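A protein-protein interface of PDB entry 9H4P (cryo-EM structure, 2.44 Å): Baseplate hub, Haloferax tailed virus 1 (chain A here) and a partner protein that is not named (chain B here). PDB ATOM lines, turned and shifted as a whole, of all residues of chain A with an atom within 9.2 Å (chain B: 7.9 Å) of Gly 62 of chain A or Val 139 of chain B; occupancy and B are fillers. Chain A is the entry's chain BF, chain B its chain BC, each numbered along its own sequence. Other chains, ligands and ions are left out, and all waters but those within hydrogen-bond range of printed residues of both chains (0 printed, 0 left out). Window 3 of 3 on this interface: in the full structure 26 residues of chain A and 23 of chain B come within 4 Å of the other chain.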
ATOM      1  N   ASP A  59      10.832 -12.771 -22.774  1.00  0.00           N
ATOM      2  CA  ASP A  59      10.540 -13.757 -21.740  1.00  0.00           C
ATOM      3  C   ASP A  59       9.314 -13.371 -20.933  1.00  0.00           C
ATOM      4  O   ASP A  59       9.032 -12.192 -20.745  1.00  0.00           O
ATOM      5  CB  ASP A  59      11.723 -13.894 -20.794  1.00  0.00           C
ATOM      6  CG  ASP A  59      12.801 -14.753 -21.417  1.00  0.00           C
ATOM      7  OD1 ASP A  59      12.611 -15.985 -21.463  1.00  0.00           O
ATOM      8  OD2 ASP A  59      13.824 -14.195 -21.875  1.00  0.00           O
ATOM      9  N   ASP A  60       8.626 -14.365 -20.386  1.00  0.00           N
ATOM     10  CA  ASP A  60       7.527 -14.159 -19.460  1.00  0.00           C
ATOM     11  C   ASP A  60       7.559 -15.168 -18.300  1.00  0.00           C
ATOM     12  O   ASP A  60       8.303 -16.153 -18.326  1.00  0.00           O
ATOM     13  CB  ASP A  60       6.208 -14.146 -20.241  1.00  0.00           C
ATOM     14  CG  ASP A  60       5.060 -13.503 -19.456  1.00  0.00           C
ATOM     15  OD1 ASP A  60       5.324 -12.942 -18.370  1.00  0.00           O
ATOM     16  OD2 ASP A  60       3.917 -13.462 -19.948  1.00  0.00           O
ATOM     17  N   ARG A  61       6.805 -14.890 -17.240  1.00  0.00           N
ATOM     18  CA  ARG A  61       6.684 -15.649 -15.996  1.00  0.00           C
ATOM     19  C   ARG A  61       5.233 -15.618 -15.559  1.00  0.00           C
ATOM     20  O   ARG A  61       4.682 -14.537 -15.390  1.00  0.00           O
ATOM     21  CB  ARG A  61       7.529 -14.947 -14.934  1.00  0.00           C
ATOM     22  CG  ARG A  61       9.028 -15.065 -15.196  1.00  0.00           C
ATOM     23  CD  ARG A  61       9.798 -13.981 -14.461  1.00  0.00           C
ATOM     24  NE  ARG A  61       9.419 -12.637 -14.929  1.00  0.00           N
ATOM     25  CZ  ARG A  61       9.749 -12.057 -16.064  1.00  0.00           C
ATOM     26  NH1 ARG A  61       9.203 -10.923 -16.373  1.00  0.00           N
ATOM     27  NH2 ARG A  61      10.610 -12.557 -16.893  1.00  0.00           N
ATOM     28  N   GLY A  62       4.600 -16.768 -15.363  1.00  0.00           N
ATOM     29  CA  GLY A  62       3.234 -16.829 -14.843  1.00  0.00           C
ATOM     30  C   GLY A  62       2.227 -16.059 -15.701  1.00  0.00           C
ATOM     31  O   GLY A  62       1.263 -15.519 -15.169  1.00  0.00           O
ATOM     32  N   GLY A  63       2.479 -15.933 -17.005  1.00  0.00           N
ATOM     33  CA  GLY A  63       1.639 -15.165 -17.923  1.00  0.00           C
ATOM     34  C   GLY A  63       1.544 -13.666 -17.623  1.00  0.00           C
ATOM     35  O   GLY A  63       0.606 -13.017 -18.084  1.00  0.00           O
ATOM     36  N   GLN A  64       2.440 -13.098 -16.816  1.00  0.00           N
ATOM     37  CA  GLN A  64       2.330 -11.720 -16.354  1.00  0.00           C
ATOM     38  C   GLN A  64       2.476 -10.699 -17.483  1.00  0.00           C
ATOM     39  O   GLN A  64       1.752  -9.708 -17.496  1.00  0.00           O
ATOM     40  CB  GLN A  64       3.379 -11.452 -15.276  1.00  0.00           C
ATOM     41  CG  GLN A  64       3.058 -12.151 -13.952  1.00  0.00           C
ATOM     42  CD  GLN A  64       4.228 -12.145 -12.976  1.00  0.00           C
ATOM     43  OE1 GLN A  64       5.212 -11.433 -13.117  1.00  0.00           O
ATOM     44  NE2 GLN A  64       4.165 -12.919 -11.921  1.00  0.00           N
ATOM     45  N   ALA A  65       3.379 -10.909 -18.434  1.00  0.00           N
ATOM     46  CA  ALA A  65       3.499 -10.039 -19.593  1.00  0.00           C
ATOM     47  C   ALA A  65       2.435 -10.340 -20.649  1.00  0.00           C
ATOM     48  O   ALA A  65       1.946  -9.397 -21.256  1.00  0.00           O
ATOM     49  CB  ALA A  65       4.915 -10.104 -20.169  1.00  0.00           C
ATOM     50  N   PHE A  66       2.000 -11.587 -20.851  1.00  0.00           N
ATOM     51  CA  PHE A  66       0.933 -11.908 -21.809  1.00  0.00           C
ATOM     52  C   PHE A  66      -0.345 -11.125 -21.500  1.00  0.00           C
ATOM     53  O   PHE A  66      -1.037 -10.661 -22.401  1.00  0.00           O
ATOM     54  CB  PHE A  66       0.683 -13.421 -21.798  1.00  0.00           C
ATOM     55  CG  PHE A  66      -0.453 -13.926 -22.671  1.00  0.00           C
ATOM     56  CD1 PHE A  66      -1.769 -13.940 -22.179  1.00  0.00           C
ATOM     57  CD2 PHE A  66      -0.196 -14.446 -23.949  1.00  0.00           C
ATOM     58  CE1 PHE A  66      -2.815 -14.456 -22.959  1.00  0.00           C
ATOM     59  CE2 PHE A  66      -1.241 -14.971 -24.724  1.00  0.00           C
ATOM     60  CZ  PHE A  66      -2.553 -14.966 -24.235  1.00  0.00           C
ATOM     61  N   GLU A  67      -0.634 -10.902 -20.222  1.00  0.00           N
ATOM     62  CA  GLU A  67      -1.753 -10.096 -19.749  1.00  0.00           C
ATOM     63  C   GLU A  67      -1.695  -8.614 -20.179  1.00  0.00           C
ATOM     64  O   GLU A  67      -2.725  -7.950 -20.228  1.00  0.00           O
ATOM     65  CB  GLU A  67      -1.807 -10.249 -18.224  1.00  0.00           C
ATOM     66  CG  GLU A  67      -3.060  -9.636 -17.597  1.00  0.00           C
ATOM     67  CD  GLU A  67      -3.238 -10.025 -16.121  1.00  0.00           C
ATOM     68  OE1 GLU A  67      -2.241 -10.071 -15.364  1.00  0.00           O
ATOM     69  OE2 GLU A  67      -4.393 -10.269 -15.703  1.00  0.00           O
ATOM     70  N   GLU A  99       2.026 -17.175 -26.190  1.00  0.00           N
ATOM     71  CA  GLU A  99       3.042 -17.651 -25.274  1.00  0.00           C
ATOM     72  C   GLU A  99       3.129 -19.161 -25.333  1.00  0.00           C
ATOM     73  O   GLU A  99       2.127 -19.857 -25.187  1.00  0.00           O
ATOM     74  CB  GLU A  99       2.774 -17.121 -23.874  1.00  0.00           C
ATOM     75  CG  GLU A  99       3.949 -17.368 -22.928  1.00  0.00           C
ATOM     76  CD  GLU A  99       3.639 -16.959 -21.485  1.00  0.00           C
ATOM     77  OE1 GLU A  99       2.552 -16.401 -21.244  1.00  0.00           O
ATOM     78  OE2 GLU A  99       4.464 -17.268 -20.596  1.00  0.00           O
ATOM     79  N   ASP A 106       9.679 -19.918 -21.292  1.00  0.00           N
ATOM     80  CA  ASP A 106       8.324 -19.452 -21.600  1.00  0.00           C
ATOM     81  C   ASP A 106       8.456 -18.171 -22.418  1.00  0.00           C
ATOM     82  O   ASP A 106       8.788 -17.123 -21.865  1.00  0.00           O
ATOM     83  CB  ASP A 106       7.518 -19.194 -20.319  1.00  0.00           C
ATOM     84  CG  ASP A 106       7.566 -20.338 -19.313  1.00  0.00           C
ATOM     85  OD1 ASP A 106       7.036 -21.434 -19.599  1.00  0.00           O
ATOM     86  OD2 ASP A 106       8.200 -20.167 -18.249  1.00  0.00           O
ATOM     87  N   SER B  81      15.103 -21.365  -7.089  1.00  0.00           N
ATOM     88  CA  SER B  81      14.737 -20.206  -6.283  1.00  0.00           C
ATOM     89  C   SER B  81      15.171 -18.926  -6.997  1.00  0.00           C
ATOM     90  O   SER B  81      16.241 -18.891  -7.608  1.00  0.00           O
ATOM     91  CB  SER B  81      15.328 -20.270  -4.887  1.00  0.00           C
ATOM     92  OG  SER B  81      14.940 -19.142  -4.113  1.00  0.00           O
ATOM     93  N   THR B  82      14.351 -17.872  -6.869  1.00  0.00           N
ATOM     94  CA  THR B  82      14.670 -16.535  -7.358  1.00  0.00           C
ATOM     95  C   THR B  82      15.652 -15.801  -6.439  1.00  0.00           C
ATOM     96  O   THR B  82      16.135 -14.730  -6.809  1.00  0.00           O
ATOM     97  CB  THR B  82      13.408 -15.684  -7.558  1.00  0.00           C
ATOM     98  OG1 THR B  82      12.683 -15.606  -6.330  1.00  0.00           O
ATOM     99  CG2 THR B  82      12.499 -16.226  -8.637  1.00  0.00           C
ATOM    100  N   ARG B 137      14.942 -13.663 -12.231  1.00  0.00           N
ATOM    101  CA  ARG B 137      13.492 -13.567 -12.375  1.00  0.00           C
ATOM    102  C   ARG B 137      12.877 -14.969 -12.359  1.00  0.00           C
ATOM    103  O   ARG B 137      13.507 -15.916 -12.828  1.00  0.00           O
ATOM    104  CB  ARG B 137      13.145 -12.829 -13.677  1.00  0.00           C
ATOM    105  CG  ARG B 137      13.806 -11.465 -13.840  1.00  0.00           C
ATOM    106  CD  ARG B 137      13.256 -10.369 -12.939  1.00  0.00           C
ATOM    107  NE  ARG B 137      14.169  -9.246 -12.759  1.00  0.00           N
ATOM    108  CZ  ARG B 137      14.414  -8.289 -13.650  1.00  0.00           C
ATOM    109  NH1 ARG B 137      15.268  -7.327 -13.351  1.00  0.00           N
ATOM    110  NH2 ARG B 137      13.826  -8.289 -14.834  1.00  0.00           N
ATOM    111  N   GLY B 138      11.649 -15.100 -11.827  1.00  0.00           N
ATOM    112  CA  GLY B 138      10.960 -16.388 -11.771  1.00  0.00           C
ATOM    113  C   GLY B 138       9.601 -16.318 -11.072  1.00  0.00           C
ATOM    114  O   GLY B 138       9.284 -15.319 -10.427  1.00  0.00           O
ATOM    115  N   VAL B 139       8.806 -17.394 -11.210  1.00  0.00           N
ATOM    116  CA  VAL B 139       7.463 -17.494 -10.643  1.00  0.00           C
ATOM    117  C   VAL B 139       7.536 -17.840  -9.152  1.00  0.00           C
ATOM    118  O   VAL B 139       6.928 -17.153  -8.328  1.00  0.00           O
ATOM    119  CB  VAL B 139       6.572 -18.501 -11.411  1.00  0.00           C
ATOM    120  CG1 VAL B 139       5.216 -18.729 -10.755  1.00  0.00           C
ATOM    121  CG2 VAL B 139       6.385 -18.137 -12.875  1.00  0.00           C
ATOM    122  N   GLY B 140       8.254 -18.923  -8.817  1.00  0.00           N
ATOM    123  CA  GLY B 140       8.236 -19.483  -7.473  1.00  0.00           C
ATOM    124  C   GLY B 140       9.252 -20.608  -7.279  1.00  0.00           C
ATOM    125  O   GLY B 140       9.790 -21.147  -8.248  1.00  0.00           O
ATOM    126  N   ASP B 141       9.480 -20.966  -6.007  1.00  0.00           N
ATOM    127  CA  ASP B 141      10.550 -21.862  -5.584  1.00  0.00           C
ATOM    128  C   ASP B 141      10.140 -23.333  -5.702  1.00  0.00           C
ATOM    129  O   ASP B 141       8.961 -23.669  -5.583  1.00  0.00           O
ATOM    130  CB  ASP B 141      10.976 -21.567  -4.141  1.00  0.00           C
ATOM    131  CG  ASP B 141      11.250 -20.104  -3.845  1.00  0.00           C
ATOM    132  OD1 ASP B 141      10.283 -19.338  -3.725  1.00  0.00           O
ATOM    133  OD2 ASP B 141      12.427 -19.752  -3.726  1.00  0.00           O
ATOM    134  N   GLU B 196      16.373 -16.466 -15.997  1.00  0.00           N
ATOM    135  CA  GLU B 196      14.983 -16.867 -15.816  1.00  0.00           C
ATOM    136  C   GLU B 196      14.938 -18.237 -15.131  1.00  0.00           C
ATOM    137  O   GLU B 196      15.185 -19.265 -15.769  1.00  0.00           O
ATOM    138  CB  GLU B 196      14.258 -16.911 -17.169  1.00  0.00           C
ATOM    139  CG  GLU B 196      14.284 -15.604 -17.950  1.00  0.00           C
ATOM    140  CD  GLU B 196      13.455 -14.472 -17.368  1.00  0.00           C
ATOM    141  OE1 GLU B 196      12.375 -14.749 -16.825  1.00  0.00           O
ATOM    142  OE2 GLU B 196      13.890 -13.317 -17.458  1.00  0.00           O
ATOM    143  N   VAL B 197      14.627 -18.236 -13.824  1.00  0.00           N
ATOM    144  CA  VAL B 197      14.505 -19.436 -12.998  1.00  0.00           C
ATOM    145  C   VAL B 197      13.139 -20.083 -13.253  1.00  0.00           C
ATOM    146  O   VAL B 197      12.114 -19.413 -13.113  1.00  0.00           O
ATOM    147  CB  VAL B 197      14.678 -19.100 -11.498  1.00  0.00           C
ATOM    148  CG1 VAL B 197      14.481 -20.316 -10.599  1.00  0.00           C
ATOM    149  CG2 VAL B 197      16.009 -18.429 -11.188  1.00  0.00           C
ATOM    150  N   LYS B 198      13.132 -21.392 -13.568  1.00  0.00           N
ATOM    151  CA  LYS B 198      11.917 -22.109 -13.940  1.00  0.00           C
ATOM    152  C   LYS B 198      11.630 -23.250 -12.963  1.00  0.00           C
ATOM    153  O   LYS B 198      12.498 -24.086 -12.713  1.00  0.00           O
ATOM    154  CB  LYS B 198      12.013 -22.628 -15.383  1.00  0.00           C
ATOM    155  CG  LYS B 198      12.169 -21.562 -16.463  1.00  0.00           C
ATOM    156  CD  LYS B 198      11.059 -20.526 -16.454  1.00  0.00           C
ATOM    157  CE  LYS B 198      11.238 -19.446 -17.499  1.00  0.00           C
ATOM    158  NZ  LYS B 198      10.078 -18.522 -17.528  1.00  0.00           N
ATOM    159  N   ALA B 199      10.391 -23.290 -12.443  1.00  0.00           N
ATOM    160  CA  ALA B 199       9.870 -24.419 -11.681  1.00  0.00           C
ATOM    161  C   ALA B 199       9.525 -25.573 -12.633  1.00  0.00           C
ATOM    162  O   ALA B 199       8.352 -25.905 -12.818  1.00  0.00           O
ATOM    163  CB  ALA B 199       8.681 -23.971 -10.856  1.00  0.00           C
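Among the printed residues, pairs that only touch across the chains: Gly 62 of chain A with Val 139 of chain B (3.4 Å), Arg 61 of chain A with Gly 138 of chain B (3.4 Å), Arg 61 of chain A with Arg 137 of chain B (3.6 Å), Arg 61 of chain A with Val 139 of chain B (3.9 Å) and Asp 59 of chain A with Glu 196 of chain B (3.9 Å).
The backbone NH of Val 197 of chain B is in hydrogen-bond range of the backbone carbonyl oxygen of Arg 137 of chain B.
The backbone NH (N) of Gln 64 of chain A lies within hydrogen-bond range of the side-chain carboxylate (OD1) of Asp 60 of chain A.
OD1 of Asp 60 of chain A lies within hydrogen-bond range of N of Ala 65 of chain A, 2.8 Å away.
OD2 of Asp 60 of chain A is in hydrogen-bond range of N of Phe 66 of chain A (2.8 Å).
N of Asp 60 of chain A lies within hydrogen-bond range of O of Asp 106 of chain A (3.1 Å).
Of the 11 printed residues of chain B, 5 touch a printed residue of chain A.
Hydrophobic or aromatic side chains of chain B within 4 Å of the printed part of chain A: Val 139.
Of the printed residues of chain B, Asp 60 of chain A touches Lys 198 (3.1 Å).
Of the printed residues of chain B, Arg 61 of chain A touches Arg 137, Gly 138, Val 139 and Glu 196.
Gly 62 of chain A touches just one residue of chain B: Val 139 (3.4 Å).
Ser 81 of chain B touches none of the printed residues of chain A.
Thr 82 of chain B touches none of the printed residues of chain A.
Printed residues of chain A within 4 Å of Gly 138 of chain B: Arg 61.
Of the printed residues of chain A, Val 139 of chain B touches Arg 61 and Gly 62.
Gly 140 of chain B touches none of the printed residues of chain A.
Of the printed residues of chain A, Lys 198 of chain B touches Asp 60 (3.1 Å) and Asp 106 (2.6 Å).
The nearest residue of chain A that does not touch Val 139 of chain B is Gln 64 of chain A (5.8 Å).
The nearest printed residue of chain A that does not touch Arg 137 of chain B is Asp 59 of chain A (7.3 Å).
The side-chain carboxylate (OD2) of Asp 106 of chain A is in salt-bridge range of the side-chain amino group (NZ) of Lys 198 of chain B.
NH2 of Arg 61 of chain A lies within salt-bridge range of OE1 of Glu 196 of chain B (2.8 Å).
The side-chain amino group of Lys 198 of chain B is in hydrogen-bond range of the backbone carbonyl oxygen of Asp 60 of chain A.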
